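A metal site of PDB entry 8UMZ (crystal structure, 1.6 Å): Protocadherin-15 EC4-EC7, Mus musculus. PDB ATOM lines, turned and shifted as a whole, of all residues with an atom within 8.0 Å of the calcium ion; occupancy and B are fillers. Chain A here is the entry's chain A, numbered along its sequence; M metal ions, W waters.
Residues that only touch the calcium ion: Gln 103 (3.9 Å).
Within 4 Å of the calcium ion: Asn 4, Gln 6, Asp 45, Asp 47, Asp 100 and Gln 103.
The nearest printed residue that does not touch the calcium ion is Ser 7 (4.6 Å).
The side-chain amide nitrogen (NE2) of Gln 103 sits at hydrogen-bond distance from the backbone carbonyl oxygen (O) of Asn 4 (3.2 Å).
The side-chain amide oxygen (OD1) of Asn 5 sits close to the side-chain carboxylate (OD1) of Asp 47 (3.1 Å).
The side-chain amide oxygen (OD1) of Asn 5 lies close to the side-chain amide nitrogen (NE2) of Gln 6 (3.4 Å).
OD1 of Asp 100 is in hydrogen-bond range of N of Val 102 (2.9 Å).
The backbone NH (N) of Gln 103 is in hydrogen-bond range of the side-chain carboxylate (OD1) of Asp 100 (2.8 Å).
The calcium ion is bound by O of Gln 6, OD2 of Asp 47, OD2 of Asp 45, OD2 of Asp 100, OD1 of Asn 4, water W1 and OD1 of Asp 45.
The calcium ion has seven donor atoms within binding distance.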
ATOM      1  N   GLU A   3     -14.155  16.746 -25.558  1.00  0.00           N
ATOM      2  CA  GLU A   3     -14.427  16.935 -27.015  1.00  0.00           C
ATOM      3  C   GLU A   3     -15.681  16.116 -27.368  1.00  0.00           C
ATOM      4  O   GLU A   3     -16.739  16.480 -26.859  1.00  0.00           O
ATOM      5  CB  GLU A   3     -13.133  16.686 -27.788  1.00  0.00           C
ATOM      6  CG  GLU A   3     -12.162  17.841 -27.571  1.00  0.00           C
ATOM      7  CD  GLU A   3     -10.676  17.548 -27.664  1.00  0.00           C
ATOM      8  OE1 GLU A   3     -10.283  16.730 -28.524  1.00  0.00           O
ATOM      9  OE2 GLU A   3      -9.908  18.175 -26.899  1.00  0.00           O
ATOM     10  N   ASN A   4     -15.574  15.042 -28.156  1.00  0.00           N
ATOM     11  CA  ASN A   4     -16.769  14.468 -28.775  1.00  0.00           C
ATOM     12  C   ASN A   4     -16.550  13.005 -29.112  1.00  0.00           C
ATOM     13  O   ASN A   4     -16.398  12.645 -30.285  1.00  0.00           O
ATOM     14  CB  ASN A   4     -17.161  15.286 -30.009  1.00  0.00           C
ATOM     15  CG  ASN A   4     -18.557  14.928 -30.468  1.00  0.00           C
ATOM     16  OD1 ASN A   4     -19.204  14.065 -29.856  1.00  0.00           O
ATOM     17  ND2 ASN A   4     -19.030  15.644 -31.466  1.00  0.00           N
ATOM     18  N   ASN A   5     -16.570  12.177 -28.037  1.00  0.00           N
ATOM     19  CA  ASN A   5     -16.347  10.742 -28.114  1.00  0.00           C
ATOM     20  C   ASN A   5     -17.504   9.912 -27.553  1.00  0.00           C
ATOM     21  O   ASN A   5     -17.364   8.699 -27.426  1.00  0.00           O
ATOM     22  CB  ASN A   5     -15.051  10.319 -27.408  1.00  0.00           C
ATOM     23  CG  ASN A   5     -15.178  10.261 -25.894  1.00  0.00           C
ATOM     24  OD1 ASN A   5     -15.839  11.079 -25.268  1.00  0.00           O
ATOM     25  ND2 ASN A   5     -14.514   9.279 -25.295  1.00  0.00           N
ATOM     26  N   GLN A   6     -18.646  10.520 -27.239  1.00  0.00           N
ATOM     27  CA  GLN A   6     -19.791   9.775 -26.754  1.00  0.00           C
ATOM     28  C   GLN A   6     -20.936   9.952 -27.754  1.00  0.00           C
ATOM     29  O   GLN A   6     -21.092  11.058 -28.266  1.00  0.00           O
ATOM     30  CB  GLN A   6     -20.200  10.302 -25.382  1.00  0.00           C
ATOM     31  CG  GLN A   6     -19.039  10.357 -24.396  1.00  0.00           C
ATOM     32  CD  GLN A   6     -18.821   9.044 -23.703  1.00  0.00           C
ATOM     33  OE1 GLN A   6     -19.726   8.485 -23.079  1.00  0.00           O
ATOM     34  NE2 GLN A   6     -17.608   8.533 -23.759  1.00  0.00           N
ATOM     35  N   SER A   7     -21.601   8.831 -28.074  1.00  0.00           N
ATOM     36  CA  SER A   7     -22.678   8.816 -29.077  1.00  0.00           C
ATOM     37  C   SER A   7     -23.908   9.391 -28.420  1.00  0.00           C
ATOM     38  O   SER A   7     -24.260   9.045 -27.296  1.00  0.00           O
ATOM     39  CB  SER A   7     -22.904   7.452 -29.601  1.00  0.00           C
ATOM     40  OG  SER A   7     -21.749   6.985 -30.305  1.00  0.00           O
ATOM     41  N   PRO A   8     -24.680  10.220 -29.128  1.00  0.00           N
ATOM     42  CA  PRO A   8     -25.932  10.761 -28.615  1.00  0.00           C
ATOM     43  C   PRO A   8     -26.935   9.634 -28.568  1.00  0.00           C
ATOM     44  O   PRO A   8     -26.741   8.589 -29.246  1.00  0.00           O
ATOM     45  CB  PRO A   8     -26.281  11.843 -29.659  1.00  0.00           C
ATOM     46  CG  PRO A   8     -25.808  11.221 -30.919  1.00  0.00           C
ATOM     47  CD  PRO A   8     -24.469  10.612 -30.535  1.00  0.00           C
ATOM     48  N   TYR A   9     -28.028   9.856 -27.816  1.00  0.00           N
ATOM     49  CA  TYR A   9     -29.044   8.821 -27.746  1.00  0.00           C
ATOM     50  C   TYR A   9     -30.400   9.381 -27.339  1.00  0.00           C
ATOM     51  O   TYR A   9     -30.520  10.330 -26.572  1.00  0.00           O
ATOM     52  CB  TYR A   9     -28.738   7.761 -26.701  1.00  0.00           C
ATOM     53  CG  TYR A   9     -28.567   8.267 -25.280  1.00  0.00           C
ATOM     54  CD1 TYR A   9     -27.395   8.901 -24.905  1.00  0.00           C
ATOM     55  CD2 TYR A   9     -29.560   8.085 -24.335  1.00  0.00           C
ATOM     56  CE1 TYR A   9     -27.239   9.403 -23.637  1.00  0.00           C
ATOM     57  CE2 TYR A   9     -29.432   8.594 -23.072  1.00  0.00           C
ATOM     58  CZ  TYR A   9     -28.260   9.222 -22.709  1.00  0.00           C
ATOM     59  OH  TYR A   9     -28.094   9.664 -21.448  1.00  0.00           O
ATOM     60  N   LEU A  44     -29.948  13.062 -25.712  1.00  0.00           N
ATOM     61  CA  LEU A  44     -28.896  13.479 -24.808  1.00  0.00           C
ATOM     62  C   LEU A  44     -27.561  13.016 -25.390  1.00  0.00           C
ATOM     63  O   LEU A  44     -27.545  12.303 -26.388  1.00  0.00           O
ATOM     64  CB  LEU A  44     -29.185  12.851 -23.430  1.00  0.00           C
ATOM     65  CG  LEU A  44     -30.477  13.246 -22.744  1.00  0.00           C
ATOM     66  CD1 LEU A  44     -30.762  12.382 -21.529  1.00  0.00           C
ATOM     67  CD2 LEU A  44     -30.457  14.729 -22.387  1.00  0.00           C
ATOM     68  N   ASP A  45     -26.467  13.481 -24.775  1.00  0.00           N
ATOM     69  CA  ASP A  45     -25.124  13.192 -25.249  1.00  0.00           C
ATOM     70  C   ASP A  45     -24.179  13.463 -24.103  1.00  0.00           C
ATOM     71  O   ASP A  45     -24.106  14.592 -23.688  1.00  0.00           O
ATOM     72  CB  ASP A  45     -24.744  14.097 -26.416  1.00  0.00           C
ATOM     73  CG  ASP A  45     -23.466  13.692 -27.098  1.00  0.00           C
ATOM     74  OD1 ASP A  45     -22.525  13.408 -26.385  1.00  0.00           O
ATOM     75  OD2 ASP A  45     -23.445  13.578 -28.356  1.00  0.00           O
ATOM     76  N   LYS A  46     -23.492  12.428 -23.684  1.00  0.00           N
ATOM     77  CA  LYS A  46     -22.721  12.456 -22.450  1.00  0.00           C
ATOM     78  C   LYS A  46     -21.449  13.261 -22.604  1.00  0.00           C
ATOM     79  O   LYS A  46     -20.765  13.476 -21.605  1.00  0.00           O
ATOM     80  CB  LYS A  46     -22.493  11.063 -21.906  1.00  0.00           C
ATOM     81  CG  LYS A  46     -23.700  10.417 -21.213  1.00  0.00           C
ATOM     82  CD  LYS A  46     -24.242  11.134 -19.985  1.00  0.00           C
ATOM     83  CE  LYS A  46     -25.030  10.207 -19.082  1.00  0.00           C
ATOM     84  NZ  LYS A  46     -25.848  10.945 -18.092  1.00  0.00           N
ATOM     85  N   ASP A  47     -21.182  13.796 -23.795  1.00  0.00           N
ATOM     86  CA  ASP A  47     -20.119  14.782 -23.915  1.00  0.00           C
ATOM     87  C   ASP A  47     -20.539  16.129 -23.318  1.00  0.00           C
ATOM     88  O   ASP A  47     -19.673  16.992 -23.087  1.00  0.00           O
ATOM     89  CB  ASP A  47     -19.676  14.967 -25.364  1.00  0.00           C
ATOM     90  CG  ASP A  47     -18.995  13.737 -25.911  1.00  0.00           C
ATOM     91  OD1 ASP A  47     -17.940  13.401 -25.363  1.00  0.00           O
ATOM     92  OD2 ASP A  47     -19.503  13.153 -26.908  1.00  0.00           O
ATOM     93  N   ILE A  48     -21.846  16.306 -23.095  1.00  0.00           N
ATOM     94  CA  ILE A  48     -22.460  17.572 -22.717  1.00  0.00           C
ATOM     95  C   ILE A  48     -23.018  17.425 -21.295  1.00  0.00           C
ATOM     96  O   ILE A  48     -23.670  16.442 -20.965  1.00  0.00           O
ATOM     97  CB  ILE A  48     -23.570  17.902 -23.732  1.00  0.00           C
ATOM     98  CG1 ILE A  48     -23.134  17.707 -25.185  1.00  0.00           C
ATOM     99  CG2 ILE A  48     -24.137  19.285 -23.454  1.00  0.00           C
ATOM    100  CD1 ILE A  48     -21.891  18.437 -25.622  1.00  0.00           C
ATOM    101  N   PRO A  54     -27.522  19.745 -25.901  1.00  0.00           N
ATOM    102  CA  PRO A  54     -26.420  19.073 -26.602  1.00  0.00           C
ATOM    103  C   PRO A  54     -26.326  19.454 -28.084  1.00  0.00           C
ATOM    104  O   PRO A  54     -25.342  19.099 -28.739  1.00  0.00           O
ATOM    105  CB  PRO A  54     -26.735  17.584 -26.387  1.00  0.00           C
ATOM    106  CG  PRO A  54     -28.271  17.539 -26.388  1.00  0.00           C
ATOM    107  CD  PRO A  54     -28.670  18.840 -25.709  1.00  0.00           C
ATOM    108  N   LEU A  56     -27.877  18.869 -30.919  1.00  0.00           N
ATOM    109  CA  LEU A  56     -27.806  17.730 -31.803  1.00  0.00           C
ATOM    110  C   LEU A  56     -28.545  18.041 -33.066  1.00  0.00           C
ATOM    111  O   LEU A  56     -29.381  18.963 -33.096  1.00  0.00           O
ATOM    112  CB  LEU A  56     -28.362  16.478 -31.136  1.00  0.00           C
ATOM    113  CG  LEU A  56     -27.660  16.046 -29.842  1.00  0.00           C
ATOM    114  CD1 LEU A  56     -28.412  14.937 -29.087  1.00  0.00           C
ATOM    115  CD2 LEU A  56     -26.270  15.586 -30.172  1.00  0.00           C
ATOM    116  N   PHE A  99     -27.438  13.147 -34.387  1.00  0.00           N
ATOM    117  CA  PHE A  99     -26.051  13.239 -34.896  1.00  0.00           C
ATOM    118  C   PHE A  99     -25.367  14.363 -34.132  1.00  0.00           C
ATOM    119  O   PHE A  99     -25.899  15.472 -34.026  1.00  0.00           O
ATOM    120  CB  PHE A  99     -26.035  13.505 -36.417  1.00  0.00           C
ATOM    121  CG  PHE A  99     -24.667  13.644 -37.089  1.00  0.00           C
ATOM    122  CD1 PHE A  99     -23.780  12.576 -37.058  1.00  0.00           C
ATOM    123  CD2 PHE A  99     -24.289  14.795 -37.762  1.00  0.00           C
ATOM    124  CE1 PHE A  99     -22.518  12.659 -37.619  1.00  0.00           C
ATOM    125  CE2 PHE A  99     -23.045  14.855 -38.384  1.00  0.00           C
ATOM    126  CZ  PHE A  99     -22.153  13.785 -38.295  1.00  0.00           C
ATOM    127  N   ASP A 100     -24.151  14.111 -33.628  1.00  0.00           N
ATOM    128  CA  ASP A 100     -23.440  15.132 -32.847  1.00  0.00           C
ATOM    129  C   ASP A 100     -22.320  15.768 -33.677  1.00  0.00           C
ATOM    130  O   ASP A 100     -21.528  16.490 -33.115  1.00  0.00           O
ATOM    131  CB  ASP A 100     -22.879  14.554 -31.540  1.00  0.00           C
ATOM    132  CG  ASP A 100     -21.850  13.455 -31.700  1.00  0.00           C
ATOM    133  OD1 ASP A 100     -21.329  13.300 -32.815  1.00  0.00           O
ATOM    134  OD2 ASP A 100     -21.612  12.647 -30.732  1.00  0.00           O
ATOM    135  N   GLY A 101     -22.276  15.513 -34.986  1.00  0.00           N
ATOM    136  CA  GLY A 101     -21.221  16.058 -35.834  1.00  0.00           C
ATOM    137  C   GLY A 101     -20.128  15.047 -36.110  1.00  0.00           C
ATOM    138  O   GLY A 101     -19.338  15.192 -37.089  1.00  0.00           O
ATOM    139  N   VAL A 102     -20.071  14.006 -35.285  1.00  0.00           N
ATOM    140  CA  VAL A 102     -19.080  12.940 -35.425  1.00  0.00           C
ATOM    141  C   VAL A 102     -19.753  11.580 -35.536  1.00  0.00           C
ATOM    142  O   VAL A 102     -19.475  10.838 -36.478  1.00  0.00           O
ATOM    143  CB  VAL A 102     -18.078  12.951 -34.280  1.00  0.00           C
ATOM    144  CG1 VAL A 102     -17.105  11.801 -34.384  1.00  0.00           C
ATOM    145  CG2 VAL A 102     -17.388  14.287 -34.235  1.00  0.00           C
ATOM    146  N   GLN A 103     -20.602  11.219 -34.573  1.00  0.00           N
ATOM    147  CA  GLN A 103     -21.224   9.909 -34.595  1.00  0.00           C
ATOM    148  C   GLN A 103     -22.728  10.107 -34.445  1.00  0.00           C
ATOM    149  O   GLN A 103     -23.213  11.100 -33.886  1.00  0.00           O
ATOM    150  CB  GLN A 103     -20.618   8.938 -33.572  1.00  0.00           C
ATOM    151  CG  GLN A 103     -20.581   9.438 -32.133  1.00  0.00           C
ATOM    152  CD  GLN A 103     -19.220   9.959 -31.748  1.00  0.00           C
ATOM    153  OE1 GLN A 103     -18.225   9.280 -31.993  1.00  0.00           O
ATOM    154  NE2 GLN A 103     -19.149  11.174 -31.194  1.00  0.00           N
HETATM  155 CA    CA M   1     -21.136  13.337 -28.554  1.00  0.00          CA
HETATM  156  O   HOH W   1     -21.325  15.833 -28.477  1.00  0.00           O
